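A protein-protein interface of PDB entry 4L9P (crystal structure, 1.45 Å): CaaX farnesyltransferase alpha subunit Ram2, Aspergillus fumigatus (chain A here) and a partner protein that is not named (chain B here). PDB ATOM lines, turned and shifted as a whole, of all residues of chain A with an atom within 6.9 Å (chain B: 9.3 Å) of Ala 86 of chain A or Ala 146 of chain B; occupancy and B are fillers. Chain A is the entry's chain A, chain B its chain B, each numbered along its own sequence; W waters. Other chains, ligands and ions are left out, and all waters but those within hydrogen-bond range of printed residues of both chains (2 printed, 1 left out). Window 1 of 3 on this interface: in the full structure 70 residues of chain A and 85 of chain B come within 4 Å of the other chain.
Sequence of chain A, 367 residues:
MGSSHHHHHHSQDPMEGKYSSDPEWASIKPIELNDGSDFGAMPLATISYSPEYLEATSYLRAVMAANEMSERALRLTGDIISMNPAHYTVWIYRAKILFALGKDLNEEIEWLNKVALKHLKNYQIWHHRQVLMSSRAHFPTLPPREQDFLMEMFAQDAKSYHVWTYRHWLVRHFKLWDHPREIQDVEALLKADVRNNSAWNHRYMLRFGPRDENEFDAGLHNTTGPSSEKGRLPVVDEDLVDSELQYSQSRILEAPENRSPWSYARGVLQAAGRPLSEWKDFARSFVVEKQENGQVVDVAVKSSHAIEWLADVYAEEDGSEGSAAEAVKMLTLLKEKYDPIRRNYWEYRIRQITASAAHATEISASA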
ATOM      1  N   ILE A  47      28.608 -28.575 -13.570  1.00  0.00           N
ATOM      2  CA  ILE A  47      27.349 -29.290 -13.384  1.00  0.00           C
ATOM      3  C   ILE A  47      27.141 -30.172 -14.605  1.00  0.00           C
ATOM      4  O   ILE A  47      27.232 -29.704 -15.751  1.00  0.00           O
ATOM      5  CB  ILE A  47      26.148 -28.322 -13.212  1.00  0.00           C
ATOM      6  CG1 ILE A  47      26.372 -27.454 -11.962  1.00  0.00           C
ATOM      7  CG2 ILE A  47      24.839 -29.110 -13.067  1.00  0.00           C
ATOM      8  CD1 ILE A  47      25.488 -26.180 -11.970  1.00  0.00           C
ATOM      9  N   TYR A  53      18.392 -29.823 -20.830  1.00  0.00           N
ATOM     10  CA  TYR A  53      18.816 -28.481 -20.457  1.00  0.00           C
ATOM     11  C   TYR A  53      19.985 -28.031 -21.334  1.00  0.00           C
ATOM     12  O   TYR A  53      20.038 -26.865 -21.739  1.00  0.00           O
ATOM     13  CB  TYR A  53      19.182 -28.478 -18.965  1.00  0.00           C
ATOM     14  CG  TYR A  53      19.522 -27.096 -18.394  1.00  0.00           C
ATOM     15  CD1 TYR A  53      18.501 -26.198 -18.056  1.00  0.00           C
ATOM     16  CD2 TYR A  53      20.849 -26.690 -18.224  1.00  0.00           C
ATOM     17  CE1 TYR A  53      18.762 -24.967 -17.519  1.00  0.00           C
ATOM     18  CE2 TYR A  53      21.148 -25.447 -17.632  1.00  0.00           C
ATOM     19  CZ  TYR A  53      20.104 -24.597 -17.307  1.00  0.00           C
ATOM     20  OH  TYR A  53      20.404 -23.408 -16.714  1.00  0.00           O
ATOM     21  N   ILE A  80      12.922 -23.255 -20.462  1.00  0.00           N
ATOM     22  CA  ILE A  80      14.112 -23.162 -19.627  1.00  0.00           C
ATOM     23  C   ILE A  80      13.733 -22.783 -18.202  1.00  0.00           C
ATOM     24  O   ILE A  80      14.282 -23.321 -17.257  1.00  0.00           O
ATOM     25  CB  ILE A  80      15.127 -22.152 -20.198  1.00  0.00           C
ATOM     26  CG1 ILE A  80      15.721 -22.789 -21.499  1.00  0.00           C
ATOM     27  CG2 ILE A  80      16.268 -21.894 -19.162  1.00  0.00           C
ATOM     28  CD1 ILE A  80      16.560 -21.875 -22.312  1.00  0.00           C
ATOM     29  N   ILE A  81      12.803 -21.859 -18.044  1.00  0.00           N
ATOM     30  CA  ILE A  81      12.299 -21.510 -16.702  1.00  0.00           C
ATOM     31  C   ILE A  81      11.700 -22.701 -15.969  1.00  0.00           C
ATOM     32  O   ILE A  81      11.900 -22.817 -14.729  1.00  0.00           O
ATOM     33  CB  ILE A  81      11.304 -20.299 -16.776  1.00  0.00           C
ATOM     34  CG1 ILE A  81      12.115 -19.036 -17.058  1.00  0.00           C
ATOM     35  CG2 ILE A  81      10.459 -20.165 -15.472  1.00  0.00           C
ATOM     36  CD1 ILE A  81      11.259 -17.821 -17.526  1.00  0.00           C
ATOM     37  N   MET A  83      12.752 -25.688 -16.184  1.00  0.00           N
ATOM     38  CA  MET A  83      13.899 -26.486 -15.713  1.00  0.00           C
ATOM     39  C   MET A  83      14.733 -25.799 -14.655  1.00  0.00           C
ATOM     40  O   MET A  83      15.265 -26.456 -13.757  1.00  0.00           O
ATOM     41  CB  MET A  83      14.799 -26.890 -16.890  1.00  0.00           C
ATOM     42  CG  MET A  83      14.117 -27.945 -17.795  1.00  0.00           C
ATOM     43  SD  MET A  83      15.205 -28.394 -19.165  1.00  0.00           S
ATOM     44  CE  MET A  83      14.946 -27.046 -20.251  1.00  0.00           C
ATOM     45  N   ASN A  84      14.841 -24.477 -14.743  1.00  0.00           N
ATOM     46  CA  ASN A  84      15.705 -23.690 -13.851  1.00  0.00           C
ATOM     47  C   ASN A  84      15.161 -22.272 -13.718  1.00  0.00           C
ATOM     48  O   ASN A  84      15.516 -21.383 -14.495  1.00  0.00           O
ATOM     49  CB  ASN A  84      17.121 -23.649 -14.378  1.00  0.00           C
ATOM     50  CG  ASN A  84      18.038 -22.826 -13.503  1.00  0.00           C
ATOM     51  OD1 ASN A  84      17.656 -22.410 -12.385  1.00  0.00           O
ATOM     52  ND2 ASN A  84      19.250 -22.557 -14.001  1.00  0.00           N
ATOM     53  N   PRO A  85      14.279 -22.057 -12.751  1.00  0.00           N
ATOM     54  CA  PRO A  85      13.676 -20.729 -12.613  1.00  0.00           C
ATOM     55  C   PRO A  85      14.676 -19.726 -12.018  1.00  0.00           C
ATOM     56  O   PRO A  85      14.355 -18.549 -11.964  1.00  0.00           O
ATOM     57  CB  PRO A  85      12.517 -20.957 -11.622  1.00  0.00           C
ATOM     58  CG  PRO A  85      12.943 -22.097 -10.823  1.00  0.00           C
ATOM     59  CD  PRO A  85      13.691 -23.025 -11.799  1.00  0.00           C
ATOM     60  N   ALA A  86      15.855 -20.161 -11.624  1.00  0.00           N
ATOM     61  CA  ALA A  86      16.887 -19.222 -11.147  1.00  0.00           C
ATOM     62  C   ALA A  86      17.885 -18.820 -12.246  1.00  0.00           C
ATOM     63  O   ALA A  86      18.985 -18.339 -11.973  1.00  0.00           O
ATOM     64  CB  ALA A  86      17.622 -19.829  -9.934  1.00  0.00           C
ATOM     65  N   HIS A  87      17.497 -18.983 -13.512  1.00  0.00           N
ATOM     66  CA  HIS A  87      18.361 -18.550 -14.625  1.00  0.00           C
ATOM     67  C   HIS A  87      18.025 -17.098 -14.894  1.00  0.00           C
ATOM     68  O   HIS A  87      17.057 -16.801 -15.600  1.00  0.00           O
ATOM     69  CB  HIS A  87      18.018 -19.461 -15.809  1.00  0.00           C
ATOM     70  CG  HIS A  87      18.949 -19.361 -16.975  1.00  0.00           C
ATOM     71  ND1 HIS A  87      19.112 -18.207 -17.724  1.00  0.00           N
ATOM     72  CD2 HIS A  87      19.690 -20.326 -17.594  1.00  0.00           C
ATOM     73  CE1 HIS A  87      19.963 -18.456 -18.707  1.00  0.00           C
ATOM     74  NE2 HIS A  87      20.351 -19.731 -18.635  1.00  0.00           N
ATOM     75  N   TYR A  88      18.786 -16.157 -14.326  1.00  0.00           N
ATOM     76  CA  TYR A  88      18.356 -14.740 -14.383  1.00  0.00           C
ATOM     77  C   TYR A  88      18.342 -14.239 -15.834  1.00  0.00           C
ATOM     78  O   TYR A  88      17.511 -13.370 -16.178  1.00  0.00           O
ATOM     79  CB  TYR A  88      19.258 -13.838 -13.476  1.00  0.00           C
ATOM     80  CG  TYR A  88      20.723 -13.875 -13.824  1.00  0.00           C
ATOM     81  CD1 TYR A  88      21.246 -13.007 -14.797  1.00  0.00           C
ATOM     82  CD2 TYR A  88      21.566 -14.840 -13.269  1.00  0.00           C
ATOM     83  CE1 TYR A  88      22.552 -13.022 -15.154  1.00  0.00           C
ATOM     84  CE2 TYR A  88      22.900 -14.897 -13.638  1.00  0.00           C
ATOM     85  CZ  TYR A  88      23.390 -13.985 -14.611  1.00  0.00           C
ATOM     86  OH  TYR A  88      24.704 -14.092 -15.016  1.00  0.00           O
ATOM     87  N   THR A  89      19.286 -14.704 -16.650  1.00  0.00           N
ATOM     88  CA  THR A  89      19.344 -14.190 -18.039  1.00  0.00           C
ATOM     89  C   THR A  89      18.032 -14.507 -18.812  1.00  0.00           C
ATOM     90  O   THR A  89      17.502 -13.654 -19.511  1.00  0.00           O
ATOM     91  CB  THR A  89      20.493 -14.843 -18.785  1.00  0.00           C
ATOM     92  OG1 THR A  89      21.726 -14.530 -18.112  1.00  0.00           O
ATOM     93  CG2 THR A  89      20.598 -14.337 -20.243  1.00  0.00           C
ATOM     94  N   VAL A  90      17.505 -15.715 -18.639  1.00  0.00           N
ATOM     95  CA  VAL A  90      16.343 -16.085 -19.486  1.00  0.00           C
ATOM     96  C   VAL A  90      15.118 -15.252 -19.112  1.00  0.00           C
ATOM     97  O   VAL A  90      14.296 -14.922 -19.970  1.00  0.00           O
ATOM     98  CB  VAL A  90      16.062 -17.586 -19.391  1.00  0.00           C
ATOM     99  CG1 VAL A  90      15.398 -17.984 -18.111  1.00  0.00           C
ATOM    100  CG2 VAL A  90      15.121 -18.015 -20.553  1.00  0.00           C
ATOM    101  N   TRP A  91      14.977 -14.838 -17.837  1.00  0.00           N
ATOM    102  CA  TRP A  91      13.832 -13.988 -17.480  1.00  0.00           C
ATOM    103  C   TRP A  91      13.946 -12.605 -18.118  1.00  0.00           C
ATOM    104  O   TRP A  91      12.945 -12.032 -18.574  1.00  0.00           O
ATOM    105  CB  TRP A  91      13.822 -13.786 -15.941  1.00  0.00           C
ATOM    106  CG  TRP A  91      13.336 -14.938 -15.178  1.00  0.00           C
ATOM    107  CD1 TRP A  91      14.085 -15.942 -14.537  1.00  0.00           C
ATOM    108  CD2 TRP A  91      11.975 -15.267 -14.964  1.00  0.00           C
ATOM    109  NE1 TRP A  91      13.229 -16.852 -13.933  1.00  0.00           N
ATOM    110  CE2 TRP A  91      11.933 -16.456 -14.185  1.00  0.00           C
ATOM    111  CE3 TRP A  91      10.771 -14.695 -15.381  1.00  0.00           C
ATOM    112  CZ2 TRP A  91      10.738 -17.011 -13.758  1.00  0.00           C
ATOM    113  CZ3 TRP A  91       9.576 -15.272 -14.950  1.00  0.00           C
ATOM    114  CH2 TRP A  91       9.561 -16.404 -14.144  1.00  0.00           C
ATOM    115  N   ASN A 122      12.997 -16.382  -4.616  1.00  0.00           N
ATOM    116  CA  ASN A 122      13.501 -16.232  -5.970  1.00  0.00           C
ATOM    117  C   ASN A 122      13.422 -14.768  -6.353  1.00  0.00           C
ATOM    118  O   ASN A 122      12.365 -14.149  -6.328  1.00  0.00           O
ATOM    119  CB  ASN A 122      12.695 -17.192  -6.855  1.00  0.00           C
ATOM    120  CG  ASN A 122      13.103 -17.162  -8.321  1.00  0.00           C
ATOM    121  OD1 ASN A 122      13.076 -16.091  -8.935  1.00  0.00           O
ATOM    122  ND2 ASN A 122      13.258 -18.397  -8.949  1.00  0.00           N
ATOM    123  N   GLN A 124      14.024 -13.477  -9.349  1.00  0.00           N
ATOM    124  CA  GLN A 124      13.677 -13.224 -10.732  1.00  0.00           C
ATOM    125  C   GLN A 124      12.173 -13.157 -10.850  1.00  0.00           C
ATOM    126  O   GLN A 124      11.663 -12.263 -11.526  1.00  0.00           O
ATOM    127  CB  GLN A 124      14.182 -14.396 -11.586  1.00  0.00           C
ATOM    128  CG  GLN A 124      15.716 -14.366 -11.842  1.00  0.00           C
ATOM    129  CD  GLN A 124      16.497 -14.661 -10.602  1.00  0.00           C
ATOM    130  OE1 GLN A 124      16.272 -15.682  -9.947  1.00  0.00           O
ATOM    131  NE2 GLN A 124      17.434 -13.768 -10.272  1.00  0.00           N
ATOM    132  N   TYR B 140      29.081 -31.598 -10.157  1.00  0.00           N
ATOM    133  CA  TYR B 140      27.781 -31.869  -9.534  1.00  0.00           C
ATOM    134  C   TYR B 140      26.873 -32.560 -10.542  1.00  0.00           C
ATOM    135  O   TYR B 140      26.974 -32.294 -11.732  1.00  0.00           O
ATOM    136  CB  TYR B 140      27.091 -30.556  -9.099  1.00  0.00           C
ATOM    137  CG  TYR B 140      27.814 -29.862  -7.981  1.00  0.00           C
ATOM    138  CD1 TYR B 140      29.026 -29.191  -8.195  1.00  0.00           C
ATOM    139  CD2 TYR B 140      27.299 -29.899  -6.685  1.00  0.00           C
ATOM    140  CE1 TYR B 140      29.662 -28.536  -7.143  1.00  0.00           C
ATOM    141  CE2 TYR B 140      27.933 -29.296  -5.637  1.00  0.00           C
ATOM    142  CZ  TYR B 140      29.115 -28.604  -5.861  1.00  0.00           C
ATOM    143  OH  TYR B 140      29.763 -27.999  -4.793  1.00  0.00           O
ATOM    144  N   PRO B 141      25.960 -33.416 -10.064  1.00  0.00           N
ATOM    145  CA  PRO B 141      24.971 -34.092 -10.924  1.00  0.00           C
ATOM    146  C   PRO B 141      23.907 -33.122 -11.452  1.00  0.00           C
ATOM    147  O   PRO B 141      23.817 -31.980 -10.968  1.00  0.00           O
ATOM    148  CB  PRO B 141      24.340 -35.157  -9.994  1.00  0.00           C
ATOM    149  CG  PRO B 141      24.691 -34.789  -8.663  1.00  0.00           C
ATOM    150  CD  PRO B 141      25.877 -33.868  -8.666  1.00  0.00           C
ATOM    151  N   ALA B 142      23.157 -33.579 -12.447  1.00  0.00           N
ATOM    152  CA  ALA B 142      22.126 -32.802 -13.146  1.00  0.00           C
ATOM    153  C   ALA B 142      21.150 -32.124 -12.223  1.00  0.00           C
ATOM    154  O   ALA B 142      20.668 -31.041 -12.557  1.00  0.00           O
ATOM    155  CB  ALA B 142      21.347 -33.692 -14.151  1.00  0.00           C
ATOM    156  N   SER B 143      20.843 -32.766 -11.091  1.00  0.00           N
ATOM    157  CA  SER B 143      19.863 -32.239 -10.149  1.00  0.00           C
ATOM    158  C   SER B 143      20.262 -30.903  -9.575  1.00  0.00           C
ATOM    159  O   SER B 143      19.425 -30.235  -8.952  1.00  0.00           O
ATOM    160  CB  SER B 143      19.632 -33.220  -8.976  1.00  0.00           C
ATOM    161  OG  SER B 143      20.858 -33.510  -8.326  1.00  0.00           O
ATOM    162  N   PHE B 144      21.540 -30.534  -9.722  1.00  0.00           N
ATOM    163  CA  PHE B 144      22.046 -29.246  -9.220  1.00  0.00           C
ATOM    164  C   PHE B 144      21.933 -28.108 -10.249  1.00  0.00           C
ATOM    165  O   PHE B 144      22.528 -27.054 -10.077  1.00  0.00           O
ATOM    166  CB  PHE B 144      23.505 -29.403  -8.773  1.00  0.00           C
ATOM    167  CG  PHE B 144      23.642 -30.073  -7.436  1.00  0.00           C
ATOM    168  CD1 PHE B 144      23.595 -31.433  -7.338  1.00  0.00           C
ATOM    169  CD2 PHE B 144      23.766 -29.309  -6.268  1.00  0.00           C
ATOM    170  CE1 PHE B 144      23.700 -32.039  -6.075  1.00  0.00           C
ATOM    171  CE2 PHE B 144      23.879 -29.877  -5.049  1.00  0.00           C
ATOM    172  CZ  PHE B 144      23.833 -31.237  -4.920  1.00  0.00           C
ATOM    173  N   VAL B 145      21.140 -28.321 -11.296  1.00  0.00           N
ATOM    174  CA  VAL B 145      21.016 -27.329 -12.366  1.00  0.00           C
ATOM    175  C   VAL B 145      20.642 -25.927 -11.850  1.00  0.00           C
ATOM    176  O   VAL B 145      21.052 -24.940 -12.459  1.00  0.00           O
ATOM    177  CB  VAL B 145      19.952 -27.779 -13.434  1.00  0.00           C
ATOM    178  CG1 VAL B 145      18.592 -27.999 -12.753  1.00  0.00           C
ATOM    179  CG2 VAL B 145      19.855 -26.787 -14.604  1.00  0.00           C
ATOM    180  N   ALA B 146      19.893 -25.803 -10.756  1.00  0.00           N
ATOM    181  CA  ALA B 146      19.532 -24.463 -10.255  1.00  0.00           C
ATOM    182  C   ALA B 146      20.730 -23.652  -9.819  1.00  0.00           C
ATOM    183  O   ALA B 146      20.632 -22.424  -9.651  1.00  0.00           O
ATOM    184  CB  ALA B 146      18.545 -24.578  -9.091  1.00  0.00           C
ATOM    185  N   LEU B 147      21.867 -24.311  -9.625  1.00  0.00           N
ATOM    186  CA  LEU B 147      23.095 -23.567  -9.284  1.00  0.00           C
ATOM    187  C   LEU B 147      23.829 -23.044 -10.516  1.00  0.00           C
ATOM    188  O   LEU B 147      24.865 -22.414 -10.388  1.00  0.00           O
ATOM    189  CB  LEU B 147      24.082 -24.411  -8.478  1.00  0.00           C
ATOM    190  CG  LEU B 147      23.599 -24.828  -7.081  1.00  0.00           C
ATOM    191  CD1 LEU B 147      24.556 -25.793  -6.355  1.00  0.00           C
ATOM    192  CD2 LEU B 147      23.414 -23.606  -6.237  1.00  0.00           C
ATOM    193  N   ASP B 148      23.271 -23.227 -11.718  1.00  0.00           N
ATOM    194  CA  ASP B 148      23.965 -22.783 -12.931  1.00  0.00           C
ATOM    195  C   ASP B 148      24.362 -21.320 -12.863  1.00  0.00           C
ATOM    196  O   ASP B 148      25.484 -20.955 -13.228  1.00  0.00           O
ATOM    197  CB  ASP B 148      23.015 -23.000 -14.121  1.00  0.00           C
ATOM    198  CG  ASP B 148      23.730 -23.017 -15.451  1.00  0.00           C
ATOM    199  OD1 ASP B 148      24.964 -23.203 -15.463  1.00  0.00           O
ATOM    200  OD2 ASP B 148      23.022 -22.896 -16.475  1.00  0.00           O
ATOM    201  N   ALA B 149      23.447 -20.463 -12.428  1.00  0.00           N
ATOM    202  CA  ALA B 149      23.754 -19.023 -12.377  1.00  0.00           C
ATOM    203  C   ALA B 149      24.748 -18.677 -11.264  1.00  0.00           C
ATOM    204  O   ALA B 149      25.353 -17.581 -11.276  1.00  0.00           O
ATOM    205  CB  ALA B 149      22.443 -18.209 -12.232  1.00  0.00           C
ATOM    206  N   SER B 150      24.918 -19.610 -10.322  1.00  0.00           N
ATOM    207  CA  SER B 150      25.733 -19.405  -9.108  1.00  0.00           C
ATOM    208  C   SER B 150      27.129 -20.054  -9.172  1.00  0.00           C
ATOM    209  O   SER B 150      27.825 -20.108  -8.151  1.00  0.00           O
ATOM    210  CB  SER B 150      25.050 -20.008  -7.888  1.00  0.00           C
ATOM    211  OG  SER B 150      23.937 -19.238  -7.583  1.00  0.00           O
ATOM    212  N   ARG B 151      27.540 -20.578 -10.328  1.00  0.00           N
ATOM    213  CA  ARG B 151      28.824 -21.278 -10.410  1.00  0.00           C
ATOM    214  C   ARG B 151      29.991 -20.391  -9.932  1.00  0.00           C
ATOM    215  O   ARG B 151      30.845 -20.855  -9.207  1.00  0.00           O
ATOM    216  CB  ARG B 151      29.054 -21.900 -11.770  1.00  0.00           C
ATOM    217  CG  ARG B 151      28.219 -23.192 -11.889  1.00  0.00           C
ATOM    218  CD  ARG B 151      28.489 -23.931 -13.207  1.00  0.00           C
ATOM    219  NE  ARG B 151      29.930 -24.220 -13.311  1.00  0.00           N
ATOM    220  CZ  ARG B 151      30.722 -23.851 -14.299  1.00  0.00           C
ATOM    221  NH1 ARG B 151      30.228 -23.222 -15.370  1.00  0.00           N
ATOM    222  NH2 ARG B 151      32.011 -24.186 -14.237  1.00  0.00           N
ATOM    223  N   TRP B 153      29.899 -18.078  -7.677  1.00  0.00           N
ATOM    224  CA  TRP B 153      29.804 -18.126  -6.217  1.00  0.00           C
ATOM    225  C   TRP B 153      30.380 -19.409  -5.635  1.00  0.00           C
ATOM    226  O   TRP B 153      31.047 -19.383  -4.585  1.00  0.00           O
ATOM    227  CB  TRP B 153      28.377 -18.013  -5.730  1.00  0.00           C
ATOM    228  CG  TRP B 153      27.805 -16.644  -5.690  1.00  0.00           C
ATOM    229  CD1 TRP B 153      26.644 -16.236  -6.290  1.00  0.00           C
ATOM    230  CD2 TRP B 153      28.256 -15.543  -4.894  1.00  0.00           C
ATOM    231  NE1 TRP B 153      26.378 -14.935  -5.943  1.00  0.00           N
ATOM    232  CE2 TRP B 153      27.355 -14.474  -5.096  1.00  0.00           C
ATOM    233  CE3 TRP B 153      29.315 -15.362  -4.003  1.00  0.00           C
ATOM    234  CZ2 TRP B 153      27.474 -13.247  -4.458  1.00  0.00           C
ATOM    235  CZ3 TRP B 153      29.446 -14.100  -3.372  1.00  0.00           C
ATOM    236  CH2 TRP B 153      28.522 -13.091  -3.602  1.00  0.00           C
ATOM    237  N   MET B 154      30.095 -20.562  -6.243  1.00  0.00           N
ATOM    238  CA  MET B 154      30.597 -21.838  -5.669  1.00  0.00           C
ATOM    239  C   MET B 154      32.129 -21.883  -5.680  1.00  0.00           C
ATOM    240  O   MET B 154      32.752 -22.487  -4.780  1.00  0.00           O
ATOM    241  CB  MET B 154      30.008 -23.046  -6.423  1.00  0.00           C
ATOM    242  CG  MET B 154      28.477 -22.959  -6.441  1.00  0.00           C
ATOM    243  SD  MET B 154      27.698 -24.026  -7.635  1.00  0.00           S
ATOM    244  CE  MET B 154      28.272 -25.401  -6.805  1.00  0.00           C
ATOM    245  N   TRP B 157      33.074 -19.321  -2.691  1.00  0.00           N
ATOM    246  CA  TRP B 157      32.821 -19.818  -1.316  1.00  0.00           C
ATOM    247  C   TRP B 157      33.844 -20.873  -0.945  1.00  0.00           C
ATOM    248  O   TRP B 157      34.343 -20.931   0.212  1.00  0.00           O
ATOM    249  CB  TRP B 157      31.413 -20.472  -1.213  1.00  0.00           C
ATOM    250  CG  TRP B 157      30.311 -19.444  -1.400  1.00  0.00           C
ATOM    251  CD1 TRP B 157      30.300 -18.151  -0.940  1.00  0.00           C
ATOM    252  CD2 TRP B 157      29.049 -19.663  -2.022  1.00  0.00           C
ATOM    253  NE1 TRP B 157      29.117 -17.538  -1.319  1.00  0.00           N
ATOM    254  CE2 TRP B 157      28.340 -18.446  -1.976  1.00  0.00           C
ATOM    255  CE3 TRP B 157      28.462 -20.784  -2.659  1.00  0.00           C
ATOM    256  CZ2 TRP B 157      27.057 -18.305  -2.541  1.00  0.00           C
ATOM    257  CZ3 TRP B 157      27.172 -20.644  -3.219  1.00  0.00           C
ATOM    258  CH2 TRP B 157      26.508 -19.406  -3.144  1.00  0.00           C
ATOM    259  N   GLY B 192      27.109 -15.993 -14.926  1.00  0.00           N
ATOM    260  CA  GLY B 192      27.192 -17.264 -14.257  1.00  0.00           C
ATOM    261  C   GLY B 192      27.933 -18.305 -15.097  1.00  0.00           C
ATOM    262  O   GLY B 192      28.347 -19.362 -14.561  1.00  0.00           O
ATOM    263  N   GLN B 196      25.471 -16.504 -20.307  1.00  0.00           N
ATOM    264  CA  GLN B 196      24.663 -15.824 -19.311  1.00  0.00           C
ATOM    265  C   GLN B 196      25.133 -14.368 -19.299  1.00  0.00           C
ATOM    266  O   GLN B 196      26.344 -14.084 -19.382  1.00  0.00           O
ATOM    267  CB  GLN B 196      24.823 -16.476 -17.920  1.00  0.00           C
ATOM    268  CG  GLN B 196      24.389 -17.955 -17.897  1.00  0.00           C
ATOM    269  CD  GLN B 196      24.401 -18.489 -16.469  1.00  0.00           C
ATOM    270  OE1 GLN B 196      23.821 -17.889 -15.570  1.00  0.00           O
ATOM    271  NE2 GLN B 196      25.093 -19.614 -16.255  1.00  0.00           N
ATOM    272  N   HIS B 199      26.522 -10.175 -14.471  1.00  0.00           N
ATOM    273  CA  HIS B 199      25.742  -9.879 -13.257  1.00  0.00           C
ATOM    274  C   HIS B 199      26.760  -9.434 -12.235  1.00  0.00           C
ATOM    275  O   HIS B 199      27.881 -10.015 -12.133  1.00  0.00           O
ATOM    276  CB  HIS B 199      25.046 -11.197 -12.821  1.00  0.00           C
ATOM    277  CG  HIS B 199      24.045 -11.046 -11.695  1.00  0.00           C
ATOM    278  ND1 HIS B 199      24.396 -10.730 -10.384  1.00  0.00           N
ATOM    279  CD2 HIS B 199      22.687 -11.175 -11.705  1.00  0.00           C
ATOM    280  CE1 HIS B 199      23.301 -10.726  -9.635  1.00  0.00           C
ATOM    281  NE2 HIS B 199      22.249 -11.005 -10.410  1.00  0.00           N
HETATM  282  O   HOH W   1      21.602 -16.512 -16.273  1.00  0.00           O
HETATM  283  O   HOH W   2      29.077 -26.386 -15.598  1.00  0.00           O
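The side-chain hydroxyl (OH) of Tyr 53 of chain A lies within hydrogen-bond range of the side-chain carboxylate (OD2) of Asp 148 of chain B, at 2.7 Å.
ND2 of Asn 84 of chain A lies within hydrogen-bond range of O of Val 145 of chain B (3.4 Å).
The backbone NH of Gly 192 of chain B sits at hydrogen-bond distance from the side-chain hydroxyl of Tyr 88 of chain A (3.1 Å).
The side-chain hydroxyl of Tyr 53 of chain A lies within hydrogen-bond range of the side-chain amide nitrogen of Asn 84 of chain A (3.1 Å).
The side-chain amide oxygen of Asn 84 of chain A sits at hydrogen-bond distance from the backbone NH of Ala 86 of chain A, at 3.0 Å.
O of Asp 148 of chain B lies within hydrogen-bond range of NE2 of Gln 196 of chain B (3.3 Å).
Tyr 140 of chain B touches Ile 47 of chain A.
CD1 of Ile 47 of chain A touches O of Phe 144 of chain B, 3.6 Å away.
Ile 47 of chain A touches Asp 148 of chain B (CD1 to N, 3.7 Å).
Tyr 53 of chain A touches Val 145 of chain B.
OD1 of Asn 84 of chain A touches CA of Ala 146 of chain B (3.5 Å).
Asn 84 of chain A touches Asp 148 of chain B.
CB of Ala 149 of chain B touches O of Ala 86 of chain A (3.5 Å).
Tyr 88 of chain A touches Gln 196 of chain B (CE2 to OE1, 3.7 Å).
His 199 of chain B touches Tyr 88 of chain A.
Gln 196 of chain B touches Thr 89 of chain A.
Of the printed residues of chain B, Ala 86 of chain A touches Ala 146 and Ala 149.
Of the printed residues of chain A, Ala 146 of chain B touches Asn 84 (3.5 Å) and Ala 86 (3.98 Å).
No residue of chain B comes within 4 Å of Pro 85 of chain A.
Of the printed residues of chain A, Gln 196 of chain B touches Tyr 88 (3.7 Å) and Thr 89 (3.4 Å).
Printed residues of chain A within 4 Å of Phe 144 of chain B: Ile 47 (3.6 Å).
Of the printed residues of chain B, Asn 84 of chain A touches Val 145, Ala 146 and Asp 148.
Of the printed residues of chain A, Gly 192 of chain B touches Tyr 88.
Ser 143 of chain B touches none of the printed residues of chain A.
Printed residues of chain A that touch a printed residue of chain B: Ile 47, Tyr 53, Met 83, Asn 84, Ala 86, Tyr 88 and Thr 89.
Hydrophobic or aromatic side chains of chain A that line the printed part of chain B: Ile 47, Tyr 53, Ala 86 and Tyr 88.
Hydrophobic or aromatic side chains of chain B that line the printed part of chain A: Val 145, Ala 149 and His 199.
Water W1 lies within hydrogen-bond range of the side-chain amide oxygen (OE1) of Gln 196 of chain B, the side-chain hydroxyl (OG1) of Thr 89 of chain A, a ring nitrogen (ND1) of His 87 of chain A and the backbone NH (N) of Tyr 88 of chain A.
Water W2 lies within hydrogen-bond range of N of Ile 47 of chain A and NE of Arg 151 of chain B.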
